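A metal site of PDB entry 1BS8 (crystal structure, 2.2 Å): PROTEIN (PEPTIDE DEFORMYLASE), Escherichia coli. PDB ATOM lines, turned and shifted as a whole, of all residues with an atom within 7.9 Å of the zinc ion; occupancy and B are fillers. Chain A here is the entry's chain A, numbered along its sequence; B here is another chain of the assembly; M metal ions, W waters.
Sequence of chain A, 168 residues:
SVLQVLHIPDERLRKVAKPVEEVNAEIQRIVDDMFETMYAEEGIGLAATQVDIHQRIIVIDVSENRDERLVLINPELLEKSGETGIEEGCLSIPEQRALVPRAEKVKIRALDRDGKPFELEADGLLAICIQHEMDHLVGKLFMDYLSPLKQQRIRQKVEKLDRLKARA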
ATOM      1  N   VAL A   5      10.739 -36.761  -6.925  1.00  0.00           N
ATOM      2  CA  VAL A   5      11.027 -35.354  -7.196  1.00  0.00           C
ATOM      3  C   VAL A   5       9.731 -34.535  -7.135  1.00  0.00           C
ATOM      4  O   VAL A   5       8.751 -34.844  -7.851  1.00  0.00           O
ATOM      5  CB  VAL A   5      11.671 -35.165  -8.597  1.00  0.00           C
ATOM      6  CG1 VAL A   5      11.914 -33.695  -8.880  1.00  0.00           C
ATOM      7  CG2 VAL A   5      12.992 -35.925  -8.665  1.00  0.00           C
ATOM      8  N   GLY A  45      22.150 -32.350 -12.714  1.00  0.00           N
ATOM      9  CA  GLY A  45      22.311 -31.819 -11.367  1.00  0.00           C
ATOM     10  C   GLY A  45      21.004 -32.007 -10.625  1.00  0.00           C
ATOM     11  O   GLY A  45      19.979 -32.273 -11.236  1.00  0.00           O
ATOM     12  N   LEU A  46      21.063 -32.016  -9.299  1.00  0.00           N
ATOM     13  CA  LEU A  46      19.888 -32.208  -8.447  1.00  0.00           C
ATOM     14  C   LEU A  46      20.225 -31.704  -7.040  1.00  0.00           C
ATOM     15  O   LEU A  46      21.324 -31.903  -6.556  1.00  0.00           O
ATOM     16  CB  LEU A  46      19.518 -33.682  -8.383  1.00  0.00           C
ATOM     17  CG  LEU A  46      18.263 -34.088  -7.630  1.00  0.00           C
ATOM     18  CD1 LEU A  46      17.005 -33.670  -8.407  1.00  0.00           C
ATOM     19  CD2 LEU A  46      18.281 -35.617  -7.427  1.00  0.00           C
ATOM     20  N   ALA A  47      19.311 -30.937  -6.451  1.00  0.00           N
ATOM     21  CA  ALA A  47      19.491 -30.457  -5.081  1.00  0.00           C
ATOM     22  C   ALA A  47      18.535 -31.131  -4.113  1.00  0.00           C
ATOM     23  O   ALA A  47      17.436 -31.563  -4.479  1.00  0.00           O
ATOM     24  CB  ALA A  47      19.302 -28.935  -5.017  1.00  0.00           C
ATOM     25  N   GLN A  50      14.596 -30.467  -3.862  1.00  0.00           N
ATOM     26  CA  GLN A  50      13.672 -31.047  -4.849  1.00  0.00           C
ATOM     27  C   GLN A  50      13.176 -32.434  -4.423  1.00  0.00           C
ATOM     28  O   GLN A  50      12.122 -32.880  -4.893  1.00  0.00           O
ATOM     29  CB  GLN A  50      14.356 -31.179  -6.206  1.00  0.00           C
ATOM     30  CG  GLN A  50      14.794 -29.880  -6.840  1.00  0.00           C
ATOM     31  CD  GLN A  50      15.610 -30.113  -8.102  1.00  0.00           C
ATOM     32  OE1 GLN A  50      16.845 -30.118  -8.056  1.00  0.00           O
ATOM     33  NE2 GLN A  50      14.926 -30.303  -9.223  1.00  0.00           N
ATOM     34  N   GLU A  88      17.568 -23.526 -20.105  1.00  0.00           N
ATOM     35  CA  GLU A  88      17.627 -24.486 -18.989  1.00  0.00           C
ATOM     36  C   GLU A  88      16.368 -25.308 -18.866  1.00  0.00           C
ATOM     37  O   GLU A  88      15.269 -24.818 -19.131  1.00  0.00           O
ATOM     38  CB  GLU A  88      17.846 -23.755 -17.664  1.00  0.00           C
ATOM     39  CG  GLU A  88      19.143 -23.002 -17.570  1.00  0.00           C
ATOM     40  CD  GLU A  88      19.344 -22.402 -16.191  1.00  0.00           C
ATOM     41  OE1 GLU A  88      18.560 -22.694 -15.257  1.00  0.00           O
ATOM     42  OE2 GLU A  88      20.295 -21.613 -16.028  1.00  0.00           O
ATOM     43  N   GLY A  89      16.510 -26.508 -18.307  1.00  0.00           N
ATOM     44  CA  GLY A  89      15.343 -27.234 -17.850  1.00  0.00           C
ATOM     45  C   GLY A  89      15.438 -27.585 -16.373  1.00  0.00           C
ATOM     46  O   GLY A  89      16.517 -27.586 -15.775  1.00  0.00           O
ATOM     47  N   CYS A  90      14.306 -27.957 -15.793  1.00  0.00           N
ATOM     48  CA  CYS A  90      14.258 -28.350 -14.383  1.00  0.00           C
ATOM     49  C   CYS A  90      13.384 -29.580 -14.137  1.00  0.00           C
ATOM     50  O   CYS A  90      12.273 -29.711 -14.676  1.00  0.00           O
ATOM     51  CB  CYS A  90      13.785 -27.170 -13.511  1.00  0.00           C
ATOM     52  SG  CYS A  90      13.991 -27.423 -11.729  1.00  0.00           S
ATOM     53  N   LEU A  91      13.926 -30.499 -13.362  1.00  0.00           N
ATOM     54  CA  LEU A  91      13.214 -31.703 -13.005  1.00  0.00           C
ATOM     55  C   LEU A  91      11.908 -31.386 -12.291  1.00  0.00           C
ATOM     56  O   LEU A  91      10.889 -31.999 -12.569  1.00  0.00           O
ATOM     57  CB  LEU A  91      14.110 -32.630 -12.171  1.00  0.00           C
ATOM     58  CG  LEU A  91      15.219 -33.338 -12.959  1.00  0.00           C
ATOM     59  CD1 LEU A  91      16.138 -32.324 -13.597  1.00  0.00           C
ATOM     60  CD2 LEU A  91      16.053 -34.243 -12.047  1.00  0.00           C
ATOM     61  N   SER A  92      11.896 -30.307 -11.514  1.00  0.00           N
ATOM     62  CA  SER A  92      10.706 -29.961 -10.768  1.00  0.00           C
ATOM     63  C   SER A  92       9.730 -29.136 -11.587  1.00  0.00           C
ATOM     64  O   SER A  92       8.610 -28.853 -11.149  1.00  0.00           O
ATOM     65  CB  SER A  92      11.081 -29.215  -9.490  1.00  0.00           C
ATOM     66  OG  SER A  92      12.052 -29.947  -8.793  1.00  0.00           O
ATOM     67  N   ILE A  93      10.165 -28.718 -12.768  1.00  0.00           N
ATOM     68  CA  ILE A  93       9.305 -27.982 -13.689  1.00  0.00           C
ATOM     69  C   ILE A  93       9.280 -28.736 -15.025  1.00  0.00           C
ATOM     70  O   ILE A  93       9.906 -28.291 -15.998  1.00  0.00           O
ATOM     71  CB  ILE A  93       9.810 -26.537 -13.923  1.00  0.00           C
ATOM     72  CG1 ILE A  93       9.955 -25.793 -12.591  1.00  0.00           C
ATOM     73  CG2 ILE A  93       8.821 -25.780 -14.784  1.00  0.00           C
ATOM     74  CD1 ILE A  93      10.760 -24.503 -12.690  1.00  0.00           C
ATOM     75  N   ARG A 102      22.750 -15.967 -16.183  1.00  0.00           N
ATOM     76  CA  ARG A 102      23.640 -16.571 -15.181  1.00  0.00           C
ATOM     77  C   ARG A 102      24.967 -15.853 -15.217  1.00  0.00           C
ATOM     78  O   ARG A 102      25.272 -15.182 -16.187  1.00  0.00           O
ATOM     79  CB  ARG A 102      23.867 -18.056 -15.483  1.00  0.00           C
ATOM     80  CG  ARG A 102      22.646 -18.923 -15.408  1.00  0.00           C
ATOM     81  CD  ARG A 102      22.157 -19.061 -13.968  1.00  0.00           C
ATOM     82  NE  ARG A 102      20.924 -19.836 -13.894  1.00  0.00           N
ATOM     83  CZ  ARG A 102      20.186 -20.002 -12.800  1.00  0.00           C
ATOM     84  NH1 ARG A 102      20.476 -19.348 -11.677  1.00  0.00           N
ATOM     85  NH2 ARG A 102      19.106 -20.772 -12.859  1.00  0.00           N
ATOM     86  N   CYS A 129      24.956 -24.800 -14.134  1.00  0.00           N
ATOM     87  CA  CYS A 129      24.348 -25.885 -13.361  1.00  0.00           C
ATOM     88  C   CYS A 129      24.499 -25.692 -11.845  1.00  0.00           C
ATOM     89  O   CYS A 129      23.538 -25.856 -11.105  1.00  0.00           O
ATOM     90  CB  CYS A 129      24.977 -27.202 -13.795  1.00  0.00           C
ATOM     91  SG  CYS A 129      24.259 -28.603 -12.997  1.00  0.00           S
ATOM     92  N   HIS A 132      22.124 -22.865 -10.801  1.00  0.00           N
ATOM     93  CA  HIS A 132      20.776 -23.432 -10.824  1.00  0.00           C
ATOM     94  C   HIS A 132      20.454 -24.250  -9.556  1.00  0.00           C
ATOM     95  O   HIS A 132      19.346 -24.207  -9.017  1.00  0.00           O
ATOM     96  CB  HIS A 132      20.645 -24.293 -12.093  1.00  0.00           C
ATOM     97  CG  HIS A 132      19.302 -24.912 -12.291  1.00  0.00           C
ATOM     98  ND1 HIS A 132      18.417 -24.494 -13.262  1.00  0.00           N
ATOM     99  CD2 HIS A 132      18.683 -25.926 -11.638  1.00  0.00           C
ATOM    100  CE1 HIS A 132      17.331 -25.228 -13.210  1.00  0.00           C
ATOM    101  NE2 HIS A 132      17.456 -26.107 -12.233  1.00  0.00           N
ATOM    102  N   GLU A 133      21.416 -25.059  -9.116  1.00  0.00           N
ATOM    103  CA  GLU A 133      21.154 -25.996  -8.049  1.00  0.00           C
ATOM    104  C   GLU A 133      21.245 -25.247  -6.717  1.00  0.00           C
ATOM    105  O   GLU A 133      20.508 -25.538  -5.779  1.00  0.00           O
ATOM    106  CB  GLU A 133      22.183 -27.151  -8.059  1.00  0.00           C
ATOM    107  CG  GLU A 133      22.228 -28.059  -9.289  1.00  0.00           C
ATOM    108  CD  GLU A 133      20.877 -28.517  -9.808  1.00  0.00           C
ATOM    109  OE1 GLU A 133      19.850 -28.511  -9.099  1.00  0.00           O
ATOM    110  OE2 GLU A 133      20.859 -28.920 -10.978  1.00  0.00           O
ATOM    111  N   ASP A 135      20.436 -22.178  -6.285  1.00  0.00           N
ATOM    112  CA  ASP A 135      19.134 -21.482  -6.195  1.00  0.00           C
ATOM    113  C   ASP A 135      18.064 -22.345  -5.536  1.00  0.00           C
ATOM    114  O   ASP A 135      17.172 -21.836  -4.883  1.00  0.00           O
ATOM    115  CB  ASP A 135      18.635 -21.083  -7.592  1.00  0.00           C
ATOM    116  CG  ASP A 135      19.134 -19.717  -8.031  1.00  0.00           C
ATOM    117  OD1 ASP A 135      19.942 -19.108  -7.310  1.00  0.00           O
ATOM    118  OD2 ASP A 135      18.706 -19.250  -9.108  1.00  0.00           O
ATOM    119  N   HIS A 136      18.068 -23.629  -5.860  1.00  0.00           N
ATOM    120  CA  HIS A 136      17.105 -24.584  -5.289  1.00  0.00           C
ATOM    121  C   HIS A 136      17.169 -24.598  -3.772  1.00  0.00           C
ATOM    122  O   HIS A 136      16.144 -24.688  -3.111  1.00  0.00           O
ATOM    123  CB  HIS A 136      17.379 -25.991  -5.797  1.00  0.00           C
ATOM    124  CG  HIS A 136      16.708 -26.297  -7.100  1.00  0.00           C
ATOM    125  ND1 HIS A 136      15.344 -26.275  -7.247  1.00  0.00           N
ATOM    126  CD2 HIS A 136      17.215 -26.648  -8.295  1.00  0.00           C
ATOM    127  CE1 HIS A 136      15.035 -26.610  -8.496  1.00  0.00           C
ATOM    128  NE2 HIS A 136      16.156 -26.844  -9.146  1.00  0.00           N
ATOM    129  N   LYS A 140      14.592 -20.852  -4.734  1.00  0.00           N
ATOM    130  CA  LYS A 140      14.438 -20.201  -6.045  1.00  0.00           C
ATOM    131  C   LYS A 140      14.329 -21.174  -7.210  1.00  0.00           C
ATOM    132  O   LYS A 140      15.121 -22.123  -7.323  1.00  0.00           O
ATOM    133  CB  LYS A 140      15.617 -19.293  -6.347  1.00  0.00           C
ATOM    134  CG  LYS A 140      15.750 -18.096  -5.469  1.00  0.00           C
ATOM    135  CD  LYS A 140      16.525 -17.009  -6.198  1.00  0.00           C
ATOM    136  CE  LYS A 140      15.886 -16.675  -7.534  1.00  0.00           C
ATOM    137  NZ  LYS A 140      16.275 -15.317  -8.007  1.00  0.00           N
ATOM    138  N   LEU A 141      13.473 -20.833  -8.174  1.00  0.00           N
ATOM    139  CA  LEU A 141      13.315 -21.626  -9.386  1.00  0.00           C
ATOM    140  C   LEU A 141      13.684 -20.749 -10.583  1.00  0.00           C
ATOM    141  O   LEU A 141      13.624 -19.531 -10.476  1.00  0.00           O
ATOM    142  CB  LEU A 141      11.866 -22.119  -9.506  1.00  0.00           C
ATOM    143  CG  LEU A 141      11.324 -22.868  -8.291  1.00  0.00           C
ATOM    144  CD1 LEU A 141       9.882 -23.231  -8.556  1.00  0.00           C
ATOM    145  CD2 LEU A 141      12.122 -24.130  -8.048  1.00  0.00           C
ATOM    146  N   PHE A 142      14.062 -21.349 -11.710  1.00  0.00           N
ATOM    147  CA  PHE A 142      14.577 -20.556 -12.848  1.00  0.00           C
ATOM    148  C   PHE A 142      13.493 -19.661 -13.462  1.00  0.00           C
ATOM    149  O   PHE A 142      13.775 -18.567 -13.952  1.00  0.00           O
ATOM    150  CB  PHE A 142      15.230 -21.471 -13.913  1.00  0.00           C
ATOM    151  CG  PHE A 142      14.258 -22.178 -14.823  1.00  0.00           C
ATOM    152  CD1 PHE A 142      13.611 -21.495 -15.849  1.00  0.00           C
ATOM    153  CD2 PHE A 142      14.045 -23.545 -14.707  1.00  0.00           C
ATOM    154  CE1 PHE A 142      12.752 -22.158 -16.736  1.00  0.00           C
ATOM    155  CE2 PHE A 142      13.200 -24.221 -15.599  1.00  0.00           C
ATOM    156  CZ  PHE A 142      12.546 -23.503 -16.621  1.00  0.00           C
ATOM    157  N   MET B   1      18.918 -29.927 -12.394  1.00  0.00           N
ATOM    158  CA  MET B   1      18.799 -29.364 -13.765  1.00  0.00           C
ATOM    159  C   MET B   1      18.638 -30.489 -14.768  1.00  0.00           C
ATOM    160  O   MET B   1      19.208 -31.561 -14.601  1.00  0.00           O
ATOM    161  CB  MET B   1      20.036 -28.543 -14.105  1.00  0.00           C
ATOM    162  CG  MET B   1      20.007 -27.899 -15.484  1.00  0.00           C
ATOM    163  SD  MET B   1      21.294 -26.692 -15.641  1.00  0.00           S
ATOM    164  CE  MET B   1      21.388 -26.457 -17.334  1.00  0.00           C
ATOM    165  N   ALA B   2      17.759 -30.276 -15.731  1.00  0.00           N
ATOM    166  CA  ALA B   2      17.681 -31.156 -16.903  1.00  0.00           C
ATOM    167  C   ALA B   2      18.324 -30.468 -18.117  1.00  0.00           C
ATOM    168  O   ALA B   2      17.772 -29.492 -18.671  1.00  0.00           O
ATOM    169  CB  ALA B   2      16.200 -31.482 -17.205  1.00  0.00           C
HETATM  170 ZN    ZN M   1      15.986 -27.511 -11.160  1.00  0.00          ZN
HETATM  171  O   HOH W   1      16.008 -29.658 -11.954  1.00  0.00           O
HETATM  172  O   HOH W   2      17.602 -28.361 -10.574  1.00  0.00           O
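Water W2 lies within hydrogen-bond range of the side-chain carboxylate (OE1) of Glu 133 (2.7 Å), the backbone NH (N) of Met 1 of chain B (2.7 Å) and the side-chain amide oxygen (OE1) of Gln 50 (3.2 Å).
OE1 of Gln 50 sits at hydrogen-bond distance from N of Ala 47 (3.1 Å). The side-chain sulfur of Cys 90 lies close to the backbone NH of Ser 92, 3.6 Å away. The side-chain amide nitrogen of Gln 50 sits at hydrogen-bond distance from the side-chain hydroxyl of Ser 92, at 2.9 Å. ND1 of His 132 sits at hydrogen-bond distance from OE1 of Glu 88 (2.7 Å). The backbone NH (N) of Met 1 of chain B is in hydrogen-bond range of the side-chain carboxylate (OE2) of Glu 133, at 2.6 Å. The backbone carbonyl oxygen of Gly 45 lies within hydrogen-bond range of the backbone NH of Met 1 of chain B.
Merely in contact with the zinc ion: Gln 50 and Met 1 of chain B.
The zinc ion is bound by water W2 (1.9 Å), the side-chain sulfur of Cys 90 (2.1 Å), a ring nitrogen (NE2) of His 136 (2.1 Å), water W1 (2.3 Å) and a ring nitrogen (NE2) of His 132 (2.3 Å). The zinc ion has five donor atoms within binding distance.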
